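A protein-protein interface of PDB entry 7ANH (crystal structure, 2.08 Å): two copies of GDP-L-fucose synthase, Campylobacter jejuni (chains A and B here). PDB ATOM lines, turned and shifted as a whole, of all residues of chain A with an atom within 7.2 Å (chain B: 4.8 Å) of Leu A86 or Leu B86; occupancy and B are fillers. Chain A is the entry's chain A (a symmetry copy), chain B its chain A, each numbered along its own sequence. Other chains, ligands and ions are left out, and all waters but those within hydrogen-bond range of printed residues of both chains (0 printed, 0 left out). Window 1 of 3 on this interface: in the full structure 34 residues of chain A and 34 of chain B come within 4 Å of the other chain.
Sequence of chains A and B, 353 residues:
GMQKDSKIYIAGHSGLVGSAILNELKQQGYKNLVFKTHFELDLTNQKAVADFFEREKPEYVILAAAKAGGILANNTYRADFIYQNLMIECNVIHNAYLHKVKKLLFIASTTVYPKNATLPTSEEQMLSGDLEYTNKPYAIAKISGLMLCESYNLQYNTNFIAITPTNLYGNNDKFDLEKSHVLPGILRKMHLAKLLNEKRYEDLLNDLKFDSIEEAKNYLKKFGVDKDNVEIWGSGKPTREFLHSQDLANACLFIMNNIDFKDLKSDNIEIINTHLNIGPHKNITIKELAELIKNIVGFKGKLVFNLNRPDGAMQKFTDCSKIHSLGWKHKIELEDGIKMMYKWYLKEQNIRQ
OG of Ser B144 is in hydrogen-bond range of OG of Ser A144, at 2.9 Å.
The side-chain sulfur (SG) of Cys A90 sits close to the backbone carbonyl oxygen (O) of Leu A86 (3.5 Å).
The backbone carbonyl oxygen (O) of Leu B86 sits close to the side-chain sulfur (SG) of Cys B90, at 3.5 Å.
The backbone carbonyl oxygen (O) of Met A87 is in hydrogen-bond range of the side-chain amide nitrogen (ND2) of Asn A91 (3.1 Å).
The backbone carbonyl oxygen of Ile A140 is in hydrogen-bond range of the side-chain hydroxyl of Ser A144 (3.4 Å).
Ile A82 touches Ser B144.
Cys B90 touches Tyr A83 (O to CE1, 3.7 Å).
Leu A86 touches Leu B86 (CD2 to CD2, 3.8 Å).
Cys B90 touches Met A87 (CB to SD, 3.5 Å).
Cys A90 touches Leu B86.
Cys A90 touches Met B87.
Ile A140 touches Ser B144.
Ile B82 touches Ser A144 (CD1 to O, 3.6 Å).
Ser A144 touches Leu B86 (OG to CD2, 3.9 Å).
Ile B82 touches Leu A148.
Of chain B, only Leu B86, Cys B90, Ser B144 and Leu B148 come within 4 Å of Leu A86.
Of chain A, only Leu A86, Cys A90, Ser A144 and Leu A148 come within 4 Å of Leu B86.
Of the printed residues of chain B, Met A87 touches Met B87 and Cys B90.
Printed residues of chain B within 4 Å of Met A147: Ile B82.
Of the printed residues of chain B, Cys A90 touches Tyr B83, Leu B86 and Met B87.
Printed residues of chain B within 4 Å of Tyr A83: Cys B90 (3.7 Å).
Ile A143 touches none of the printed residues of chain B.
Of the 24 printed residues of chain A, 9 touch a printed residue of chain B.
Hydrophobic or aromatic side chains of chain A that line the printed part of chain B: Ile A82, Tyr A83, Leu A86, Met A87, Ile A140, Met A147 and Leu A148.
Along chain A the printed residues that touch a printed residue of chain B span positions 82 to 148.
Hydrophobic or aromatic side chains of chain B that line the printed part of chain A: Ile B82, Tyr B83, Leu B86, Met B87 and Leu B148.
Ile A82 touches Ser B144, and with the chains exchanged Ser A144 touches Ile B82.
Ile A82 touches Leu B148, and with the chains exchanged Leu A148 touches Ile B82.
Tyr A83 touches Cys B90, and with the chains exchanged Cys A90 touches Tyr B83.
Met A87 touches Cys B90, and with the chains exchanged Cys A90 touches Met B87.
Of the 19 pairs that touch across the chains among the printed residues, 17 have their exchanged pair printed and touching as well.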
ATOM      1  N   LEU A  43      -6.241  20.234  25.875  1.00  0.00           N
ATOM      2  CA  LEU A  43      -7.251  19.596  25.025  1.00  0.00           C
ATOM      3  C   LEU A  43      -7.634  18.200  25.447  1.00  0.00           C
ATOM      4  O   LEU A  43      -8.664  17.757  24.995  1.00  0.00           O
ATOM      5  CB  LEU A  43      -6.847  19.574  23.538  1.00  0.00           C
ATOM      6  CG  LEU A  43      -6.570  20.968  22.964  1.00  0.00           C
ATOM      7  CD1 LEU A  43      -6.053  20.802  21.560  1.00  0.00           C
ATOM      8  CD2 LEU A  43      -7.811  21.839  22.981  1.00  0.00           C
ATOM      9  N   THR A  44      -6.828  17.518  26.275  1.00  0.00           N
ATOM     10  CA  THR A  44      -7.301  16.235  26.896  1.00  0.00           C
ATOM     11  C   THR A  44      -8.308  16.455  28.065  1.00  0.00           C
ATOM     12  O   THR A  44      -9.030  15.518  28.468  1.00  0.00           O
ATOM     13  CB  THR A  44      -6.139  15.338  27.315  1.00  0.00           C
ATOM     14  OG1 THR A  44      -5.451  15.860  28.480  1.00  0.00           O
ATOM     15  CG2 THR A  44      -5.127  15.163  26.136  1.00  0.00           C
ATOM     16  N   ASP A  80       0.278   6.958  25.743  1.00  0.00           N
ATOM     17  CA  ASP A  80       0.064   8.427  25.598  1.00  0.00           C
ATOM     18  C   ASP A  80      -0.384   8.762  24.202  1.00  0.00           C
ATOM     19  O   ASP A  80      -1.304   9.519  24.057  1.00  0.00           O
ATOM     20  CB  ASP A  80       1.281   9.239  25.941  1.00  0.00           C
ATOM     21  CG  ASP A  80       1.808   8.942  27.291  1.00  0.00           C
ATOM     22  OD1 ASP A  80       1.053   8.900  28.278  1.00  0.00           O
ATOM     23  OD2 ASP A  80       3.010   8.712  27.382  1.00  0.00           O
ATOM     24  N   PHE A  81       0.186   8.098  23.198  1.00  0.00           N
ATOM     25  CA  PHE A  81      -0.191   8.344  21.820  1.00  0.00           C
ATOM     26  C   PHE A  81      -1.613   7.906  21.440  1.00  0.00           C
ATOM     27  O   PHE A  81      -2.217   8.512  20.524  1.00  0.00           O
ATOM     28  CB  PHE A  81       0.826   7.746  20.833  1.00  0.00           C
ATOM     29  CG  PHE A  81       2.040   8.613  20.589  1.00  0.00           C
ATOM     30  CD1 PHE A  81       2.797   9.123  21.657  1.00  0.00           C
ATOM     31  CD2 PHE A  81       2.467   8.885  19.293  1.00  0.00           C
ATOM     32  CE1 PHE A  81       3.925   9.938  21.435  1.00  0.00           C
ATOM     33  CE2 PHE A  81       3.592   9.697  19.062  1.00  0.00           C
ATOM     34  CZ  PHE A  81       4.330  10.213  20.132  1.00  0.00           C
ATOM     35  N   ILE A  82      -2.197   6.934  22.134  1.00  0.00           N
ATOM     36  CA  ILE A  82      -3.608   6.599  21.809  1.00  0.00           C
ATOM     37  C   ILE A  82      -4.552   7.360  22.707  1.00  0.00           C
ATOM     38  O   ILE A  82      -5.533   7.975  22.240  1.00  0.00           O
ATOM     39  CB  ILE A  82      -3.910   5.088  21.769  1.00  0.00           C
ATOM     40  CG1 ILE A  82      -5.399   4.886  21.505  1.00  0.00           C
ATOM     41  CG2 ILE A  82      -3.517   4.422  23.061  1.00  0.00           C
ATOM     42  CD1 ILE A  82      -5.819   3.486  21.143  1.00  0.00           C
ATOM     43  N   TYR A  83      -4.258   7.364  24.008  1.00  0.00           N
ATOM     44  CA  TYR A  83      -5.153   8.009  24.963  1.00  0.00           C
ATOM     45  C   TYR A  83      -5.270   9.516  24.680  1.00  0.00           C
ATOM     46  O   TYR A  83      -6.362  10.073  24.693  1.00  0.00           O
ATOM     47  CB  TYR A  83      -4.664   7.764  26.411  1.00  0.00           C
ATOM     48  CG  TYR A  83      -5.344   8.618  27.407  1.00  0.00           C
ATOM     49  CD1 TYR A  83      -6.619   8.302  27.848  1.00  0.00           C
ATOM     50  CD2 TYR A  83      -4.769   9.800  27.841  1.00  0.00           C
ATOM     51  CE1 TYR A  83      -7.320   9.114  28.750  1.00  0.00           C
ATOM     52  CE2 TYR A  83      -5.441  10.604  28.757  1.00  0.00           C
ATOM     53  CZ  TYR A  83      -6.724  10.250  29.189  1.00  0.00           C
ATOM     54  OH  TYR A  83      -7.435  11.053  30.010  1.00  0.00           O
ATOM     55  N   GLN A  84      -4.158  10.205  24.437  1.00  0.00           N
ATOM     56  CA  GLN A  84      -4.280  11.710  24.351  1.00  0.00           C
ATOM     57  C   GLN A  84      -4.991  12.113  23.099  1.00  0.00           C
ATOM     58  O   GLN A  84      -5.837  12.980  23.161  1.00  0.00           O
ATOM     59  CB  GLN A  84      -2.946  12.393  24.456  1.00  0.00           C
ATOM     60  CG  GLN A  84      -2.413  12.421  25.880  1.00  0.00           C
ATOM     61  CD  GLN A  84      -1.049  13.074  25.952  1.00  0.00           C
ATOM     62  OE1 GLN A  84      -0.676  13.911  25.121  1.00  0.00           O
ATOM     63  NE2 GLN A  84      -0.289  12.681  26.931  1.00  0.00           N
ATOM     64  N   ASN A  85      -4.695  11.412  21.986  1.00  0.00           N
ATOM     65  CA  ASN A  85      -5.312  11.697  20.738  1.00  0.00           C
ATOM     66  C   ASN A  85      -6.811  11.371  20.792  1.00  0.00           C
ATOM     67  O   ASN A  85      -7.635  12.179  20.321  1.00  0.00           O
ATOM     68  CB  ASN A  85      -4.557  11.013  19.549  1.00  0.00           C
ATOM     69  CG  ASN A  85      -3.214  11.694  19.273  1.00  0.00           C
ATOM     70  OD1 ASN A  85      -3.213  12.819  18.825  1.00  0.00           O
ATOM     71  ND2 ASN A  85      -2.088  11.074  19.642  1.00  0.00           N
ATOM     72  N   LEU A  86      -7.180  10.212  21.368  1.00  0.00           N
ATOM     73  CA  LEU A  86      -8.571   9.894  21.534  1.00  0.00           C
ATOM     74  C   LEU A  86      -9.226  11.018  22.330  1.00  0.00           C
ATOM     75  O   LEU A  86     -10.301  11.502  21.953  1.00  0.00           O
ATOM     76  CB  LEU A  86      -8.820   8.537  22.247  1.00  0.00           C
ATOM     77  CG  LEU A  86      -8.541   7.307  21.379  1.00  0.00           C
ATOM     78  CD1 LEU A  86      -8.603   6.100  22.296  1.00  0.00           C
ATOM     79  CD2 LEU A  86      -9.390   7.143  20.093  1.00  0.00           C
ATOM     80  N   MET A  87      -8.626  11.425  23.418  1.00  0.00           N
ATOM     81  CA  MET A  87      -9.256  12.508  24.235  1.00  0.00           C
ATOM     82  C   MET A  87      -9.374  13.881  23.517  1.00  0.00           C
ATOM     83  O   MET A  87     -10.420  14.569  23.578  1.00  0.00           O
ATOM     84  CB  MET A  87      -8.551  12.659  25.577  1.00  0.00           C
ATOM     85  CG  MET A  87      -8.709  11.454  26.533  1.00  0.00           C
ATOM     86  SD  MET A  87     -10.453  11.085  26.922  1.00  0.00           S
ATOM     87  CE  MET A  87     -10.837  12.608  27.778  1.00  0.00           C
ATOM     88  N   ILE A  88      -8.318  14.262  22.811  1.00  0.00           N
ATOM     89  CA  ILE A  88      -8.304  15.563  22.060  1.00  0.00           C
ATOM     90  C   ILE A  88      -9.425  15.516  21.022  1.00  0.00           C
ATOM     91  O   ILE A  88     -10.287  16.409  20.967  1.00  0.00           O
ATOM     92  CB  ILE A  88      -6.936  15.817  21.372  1.00  0.00           C
ATOM     93  CG1 ILE A  88      -5.861  16.081  22.391  1.00  0.00           C
ATOM     94  CG2 ILE A  88      -7.003  17.007  20.396  1.00  0.00           C
ATOM     95  CD1 ILE A  88      -4.476  16.068  21.797  1.00  0.00           C
ATOM     96  N   GLU A  89      -9.445  14.406  20.277  1.00  0.00           N
ATOM     97  CA  GLU A  89     -10.442  14.192  19.295  1.00  0.00           C
ATOM     98  C   GLU A  89     -11.858  14.226  19.826  1.00  0.00           C
ATOM     99  O   GLU A  89     -12.706  14.925  19.244  1.00  0.00           O
ATOM    100  CB  GLU A  89     -10.187  12.930  18.499  1.00  0.00           C
ATOM    101  CG  GLU A  89      -8.892  12.982  17.663  1.00  0.00           C
ATOM    102  CD  GLU A  89      -8.444  11.598  17.248  1.00  0.00           C
ATOM    103  OE1 GLU A  89      -9.232  10.629  17.387  1.00  0.00           O
ATOM    104  OE2 GLU A  89      -7.297  11.490  16.813  1.00  0.00           O
ATOM    105  N   CYS A  90     -12.145  13.441  20.862  1.00  0.00           N
ATOM    106  CA  CYS A  90     -13.497  13.378  21.390  1.00  0.00           C
ATOM    107  C   CYS A  90     -13.915  14.734  21.962  1.00  0.00           C
ATOM    108  O   CYS A  90     -15.038  15.169  21.748  1.00  0.00           O
ATOM    109  CB  CYS A  90     -13.604  12.285  22.485  1.00  0.00           C
ATOM    110  SG  CYS A  90     -13.667  10.579  21.817  1.00  0.00           S
ATOM    111  N   ASN A  91     -13.053  15.385  22.722  1.00  0.00           N
ATOM    112  CA  ASN A  91     -13.451  16.659  23.416  1.00  0.00           C
ATOM    113  C   ASN A  91     -13.796  17.769  22.385  1.00  0.00           C
ATOM    114  O   ASN A  91     -14.852  18.395  22.500  1.00  0.00           O
ATOM    115  CB  ASN A  91     -12.338  17.200  24.356  1.00  0.00           C
ATOM    116  CG  ASN A  91     -12.085  16.323  25.601  1.00  0.00           C
ATOM    117  OD1 ASN A  91     -12.973  15.646  26.106  1.00  0.00           O
ATOM    118  ND2 ASN A  91     -10.849  16.368  26.117  1.00  0.00           N
ATOM    119  N   VAL A  92     -12.919  17.944  21.357  1.00  0.00           N
ATOM    120  CA  VAL A  92     -13.024  19.037  20.409  1.00  0.00           C
ATOM    121  C   VAL A  92     -14.176  18.706  19.475  1.00  0.00           C
ATOM    122  O   VAL A  92     -15.031  19.553  19.223  1.00  0.00           O
ATOM    123  CB  VAL A  92     -11.681  19.313  19.707  1.00  0.00           C
ATOM    124  CG1 VAL A  92     -11.835  20.349  18.606  1.00  0.00           C
ATOM    125  CG2 VAL A  92     -10.654  19.793  20.676  1.00  0.00           C
ATOM    126  N   PRO A 137      -0.844   2.596  17.696  1.00  0.00           N
ATOM    127  CA  PRO A 137      -1.828   3.254  18.561  1.00  0.00           C
ATOM    128  C   PRO A 137      -2.302   4.668  18.084  1.00  0.00           C
ATOM    129  O   PRO A 137      -3.444   5.032  18.277  1.00  0.00           O
ATOM    130  CB  PRO A 137      -1.115   3.324  19.926  1.00  0.00           C
ATOM    131  CG  PRO A 137       0.086   2.431  19.814  1.00  0.00           C
ATOM    132  CD  PRO A 137       0.375   2.189  18.408  1.00  0.00           C
ATOM    133  N   ILE A 140      -4.736   4.095  15.087  1.00  0.00           N
ATOM    134  CA  ILE A 140      -6.086   3.772  15.558  1.00  0.00           C
ATOM    135  C   ILE A 140      -6.763   4.992  16.097  1.00  0.00           C
ATOM    136  O   ILE A 140      -7.934   5.221  15.822  1.00  0.00           O
ATOM    137  CB  ILE A 140      -6.047   2.561  16.531  1.00  0.00           C
ATOM    138  CG1 ILE A 140      -5.773   1.288  15.689  1.00  0.00           C
ATOM    139  CG2 ILE A 140      -7.350   2.390  17.294  1.00  0.00           C
ATOM    140  CD1 ILE A 140      -5.025   0.204  16.430  1.00  0.00           C
ATOM    141  N   ALA A 141      -6.050   5.820  16.823  1.00  0.00           N
ATOM    142  CA  ALA A 141      -6.653   7.078  17.328  1.00  0.00           C
ATOM    143  C   ALA A 141      -7.113   7.921  16.185  1.00  0.00           C
ATOM    144  O   ALA A 141      -8.257   8.427  16.220  1.00  0.00           O
ATOM    145  CB  ALA A 141      -5.691   7.865  18.192  1.00  0.00           C
ATOM    146  N   LYS A 142      -6.276   8.021  15.136  1.00  0.00           N
ATOM    147  CA  LYS A 142      -6.714   8.755  13.953  1.00  0.00           C
ATOM    148  C   LYS A 142      -7.879   8.121  13.233  1.00  0.00           C
ATOM    149  O   LYS A 142      -8.730   8.839  12.804  1.00  0.00           O
ATOM    150  CB  LYS A 142      -5.594   9.039  12.969  1.00  0.00           C
ATOM    151  CG  LYS A 142      -4.406   9.886  13.466  1.00  0.00           C
ATOM    152  CD  LYS A 142      -4.879  11.232  13.988  1.00  0.00           C
ATOM    153  CE  LYS A 142      -3.740  12.097  14.485  1.00  0.00           C
ATOM    154  NZ  LYS A 142      -4.038  13.578  14.411  1.00  0.00           N
ATOM    155  N   ILE A 143      -7.920   6.801  13.071  1.00  0.00           N
ATOM    156  CA  ILE A 143      -9.070   6.182  12.475  1.00  0.00           C
ATOM    157  C   ILE A 143     -10.329   6.511  13.291  1.00  0.00           C
ATOM    158  O   ILE A 143     -11.401   6.798  12.751  1.00  0.00           O
ATOM    159  CB  ILE A 143      -8.894   4.640  12.340  1.00  0.00           C
ATOM    160  CG1 ILE A 143      -7.831   4.363  11.255  1.00  0.00           C
ATOM    161  CG2 ILE A 143     -10.225   3.980  11.977  1.00  0.00           C
ATOM    162  CD1 ILE A 143      -7.216   2.987  11.296  1.00  0.00           C
ATOM    163  N   SER A 144     -10.199   6.496  14.604  1.00  0.00           N
ATOM    164  CA  SER A 144     -11.303   6.893  15.442  1.00  0.00           C
ATOM    165  C   SER A 144     -11.751   8.334  15.191  1.00  0.00           C
ATOM    166  O   SER A 144     -12.974   8.618  15.213  1.00  0.00           O
ATOM    167  CB  SER A 144     -10.957   6.699  16.912  1.00  0.00           C
ATOM    168  OG  SER A 144     -11.000   5.299  17.245  1.00  0.00           O
ATOM    169  N   GLY A 145     -10.794   9.228  14.999  1.00  0.00           N
ATOM    170  CA  GLY A 145     -11.096  10.612  14.644  1.00  0.00           C
ATOM    171  C   GLY A 145     -11.848  10.741  13.349  1.00  0.00           C
ATOM    172  O   GLY A 145     -12.851  11.448  13.286  1.00  0.00           O
ATOM    173  N   MET A 147     -13.815   8.430  12.208  1.00  0.00           N
ATOM    174  CA  MET A 147     -15.104   7.825  12.393  1.00  0.00           C
ATOM    175  C   MET A 147     -15.969   8.725  13.223  1.00  0.00           C
ATOM    176  O   MET A 147     -17.142   8.897  12.910  1.00  0.00           O
ATOM    177  CB  MET A 147     -14.965   6.403  12.965  1.00  0.00           C
ATOM    178  CG  MET A 147     -16.275   5.656  13.116  1.00  0.00           C
ATOM    179  SD  MET A 147     -17.202   5.518  11.591  1.00  0.00           S
ATOM    180  CE  MET A 147     -15.962   4.866  10.480  1.00  0.00           C
ATOM    181  N   LEU A 148     -15.392   9.400  14.199  1.00  0.00           N
ATOM    182  CA  LEU A 148     -16.100  10.516  14.891  1.00  0.00           C
ATOM    183  C   LEU A 148     -16.705  11.573  13.932  1.00  0.00           C
ATOM    184  O   LEU A 148     -17.887  11.896  14.035  1.00  0.00           O
ATOM    185  CB  LEU A 148     -15.144  11.214  15.902  1.00  0.00           C
ATOM    186  CG  LEU A 148     -14.909  10.449  17.225  1.00  0.00           C
ATOM    187  CD1 LEU A 148     -13.716  10.948  18.016  1.00  0.00           C
ATOM    188  CD2 LEU A 148     -16.140  10.546  18.072  1.00  0.00           C
ATOM    189  N   ILE B  82     -19.887   5.757  19.001  1.00  0.00           N
ATOM    190  CA  ILE B  82     -18.403   5.827  19.010  1.00  0.00           C
ATOM    191  C   ILE B  82     -17.924   6.743  20.110  1.00  0.00           C
ATOM    192  O   ILE B  82     -17.016   6.393  20.893  1.00  0.00           O
ATOM    193  CB  ILE B  82     -17.773   6.156  17.642  1.00  0.00           C
ATOM    194  CG1 ILE B  82     -16.261   6.275  17.809  1.00  0.00           C
ATOM    195  CG2 ILE B  82     -18.336   7.435  17.080  1.00  0.00           C
ATOM    196  CD1 ILE B  82     -15.460   6.301  16.534  1.00  0.00           C
ATOM    197  N   TYR B  83     -18.546   7.919  20.214  1.00  0.00           N
ATOM    198  CA  TYR B  83     -18.103   8.901  21.198  1.00  0.00           C
ATOM    199  C   TYR B  83     -18.252   8.357  22.628  1.00  0.00           C
ATOM    200  O   TYR B  83     -17.355   8.502  23.451  1.00  0.00           O
ATOM    201  CB  TYR B  83     -18.890  10.223  21.033  1.00  0.00           C
ATOM    202  CG  TYR B  83     -18.705  11.156  22.165  1.00  0.00           C
ATOM    203  CD1 TYR B  83     -17.556  11.923  22.261  1.00  0.00           C
ATOM    204  CD2 TYR B  83     -19.623  11.206  23.200  1.00  0.00           C
ATOM    205  CE1 TYR B  83     -17.318  12.778  23.345  1.00  0.00           C
ATOM    206  CE2 TYR B  83     -19.414  12.071  24.271  1.00  0.00           C
ATOM    207  CZ  TYR B  83     -18.245  12.838  24.332  1.00  0.00           C
ATOM    208  OH  TYR B  83     -17.974  13.621  25.399  1.00  0.00           O
ATOM    209  N   GLN B  84     -19.385   7.741  22.958  1.00  0.00           N
ATOM    210  CA  GLN B  84     -19.582   7.387  24.415  1.00  0.00           C
ATOM    211  C   GLN B  84     -18.673   6.270  24.817  1.00  0.00           C
ATOM    212  O   GLN B  84     -18.088   6.346  25.877  1.00  0.00           O
ATOM    213  CB  GLN B  84     -21.014   7.056  24.729  1.00  0.00           C
ATOM    214  CG  GLN B  84     -21.897   8.291  24.808  1.00  0.00           C
ATOM    215  CD  GLN B  84     -23.341   7.927  25.081  1.00  0.00           C
ATOM    216  OE1 GLN B  84     -23.657   6.884  25.667  1.00  0.00           O
ATOM    217  NE2 GLN B  84     -24.226   8.769  24.638  1.00  0.00           N
ATOM    218  N   ASN B  85     -18.500   5.282  23.917  1.00  0.00           N
ATOM    219  CA  ASN B  85     -17.654   4.171  24.181  1.00  0.00           C
ATOM    220  C   ASN B  85     -16.189   4.620  24.275  1.00  0.00           C
ATOM    221  O   ASN B  85     -15.471   4.194  25.200  1.00  0.00           O
ATOM    222  CB  ASN B  85     -17.896   3.004  23.165  1.00  0.00           C
ATOM    223  CG  ASN B  85     -19.234   2.307  23.421  1.00  0.00           C
ATOM    224  OD1 ASN B  85     -19.366   1.655  24.435  1.00  0.00           O
ATOM    225  ND2 ASN B  85     -20.250   2.532  22.582  1.00  0.00           N
ATOM    226  N   LEU B  86     -15.738   5.483  23.344  1.00  0.00           N
ATOM    227  CA  LEU B  86     -14.406   6.014  23.432  1.00  0.00           C
ATOM    228  C   LEU B  86     -14.252   6.696  24.787  1.00  0.00           C
ATOM    229  O   LEU B  86     -13.251   6.479  25.483  1.00  0.00           O
ATOM    230  CB  LEU B  86     -14.060   7.019  22.301  1.00  0.00           C
ATOM    231  CG  LEU B  86     -13.817   6.373  20.934  1.00  0.00           C
ATOM    232  CD1 LEU B  86     -13.734   7.502  19.924  1.00  0.00           C
ATOM    233  CD2 LEU B  86     -12.644   5.367  20.826  1.00  0.00           C
ATOM    234  N   MET B  87     -15.193   7.520  25.167  1.00  0.00           N
ATOM    235  CA  MET B  87     -15.060   8.225  26.479  1.00  0.00           C
ATOM    236  C   MET B  87     -15.064   7.293  27.723  1.00  0.00           C
ATOM    237  O   MET B  87     -14.252   7.447  28.664  1.00  0.00           O
ATOM    238  CB  MET B  87     -16.110   9.319  26.620  1.00  0.00           C
ATOM    239  CG  MET B  87     -15.947  10.506  25.643  1.00  0.00           C
ATOM    240  SD  MET B  87     -14.332  11.339  25.806  1.00  0.00           S
ATOM    241  CE  MET B  87     -14.537  11.938  27.478  1.00  0.00           C
ATOM    242  N   ILE B  88     -15.953   6.309  27.709  1.00  0.00           N
ATOM    243  CA  ILE B  88     -16.057   5.330  28.845  1.00  0.00           C
ATOM    244  C   ILE B  88     -14.719   4.598  28.954  1.00  0.00           C
ATOM    245  O   ILE B  88     -14.095   4.560  30.028  1.00  0.00           O
ATOM    246  CB  ILE B  88     -17.214   4.318  28.631  1.00  0.00           C
ATOM    247  CG1 ILE B  88     -18.551   5.000  28.738  1.00  0.00           C
ATOM    248  CG2 ILE B  88     -17.157   3.166  29.650  1.00  0.00           C
ATOM    249  CD1 ILE B  88     -19.690   4.127  28.276  1.00  0.00           C
ATOM    250  N   GLU B  89     -14.256   4.112  27.799  1.00  0.00           N
ATOM    251  CA  GLU B  89     -13.013   3.438  27.724  1.00  0.00           C
ATOM    252  C   GLU B  89     -11.833   4.253  28.204  1.00  0.00           C
ATOM    253  O   GLU B  89     -11.038   3.748  29.016  1.00  0.00           O
ATOM    254  CB  GLU B  89     -12.761   2.872  26.342  1.00  0.00           C
ATOM    255  CG  GLU B  89     -13.766   1.776  25.935  1.00  0.00           C
ATOM    256  CD  GLU B  89     -13.769   1.556  24.439  1.00  0.00           C
ATOM    257  OE1 GLU B  89     -12.851   2.056  23.741  1.00  0.00           O
ATOM    258  OE2 GLU B  89     -14.706   0.907  23.972  1.00  0.00           O
ATOM    259  N   CYS B  90     -11.663   5.462  27.673  1.00  0.00           N
ATOM    260  CA  CYS B  90     -10.521   6.279  28.043  1.00  0.00           C
ATOM    261  C   CYS B  90     -10.581   6.648  29.526  1.00  0.00           C
ATOM    262  O   CYS B  90      -9.568   6.607  30.210  1.00  0.00           O
ATOM    263  CB  CYS B  90     -10.467   7.566  27.178  1.00  0.00           C
ATOM    264  SG  CYS B  90      -9.852   7.281  25.475  1.00  0.00           S
ATOM    265  N   ALA B 141     -14.618   1.766  18.231  1.00  0.00           N
ATOM    266  CA  ALA B 141     -14.465   2.132  19.660  1.00  0.00           C
ATOM    267  C   ALA B 141     -13.918   0.975  20.431  1.00  0.00           C
ATOM    268  O   ALA B 141     -12.966   1.163  21.221  1.00  0.00           O
ATOM    269  CB  ALA B 141     -15.772   2.586  20.275  1.00  0.00           C
ATOM    270  N   SER B 144     -10.287   0.436  19.671  1.00  0.00           N
ATOM    271  CA  SER B 144      -9.562   1.403  20.457  1.00  0.00           C
ATOM    272  C   SER B 144      -9.395   0.977  21.917  1.00  0.00           C
ATOM    273  O   SER B 144      -8.316   1.213  22.515  1.00  0.00           O
ATOM    274  CB  SER B 144     -10.232   2.767  20.382  1.00  0.00           C
ATOM    275  OG  SER B 144      -9.969   3.373  19.102  1.00  0.00           O
ATOM    276  N   LEU B 148      -5.953   0.627  23.763  1.00  0.00           N
ATOM    277  CA  LEU B 148      -5.720   1.223  25.111  1.00  0.00           C
ATOM    278  C   LEU B 148      -5.134   0.232  26.148  1.00  0.00           C
ATOM    279  O   LEU B 148      -4.124   0.529  26.783  1.00  0.00           O
ATOM    280  CB  LEU B 148      -7.040   1.837  25.662  1.00  0.00           C
ATOM    281  CG  LEU B 148      -7.441   3.200  25.050  1.00  0.00           C
ATOM    282  CD1 LEU B 148      -8.881   3.591  25.319  1.00  0.00           C
ATOM    283  CD2 LEU B 148      -6.532   4.262  25.586  1.00  0.00           C
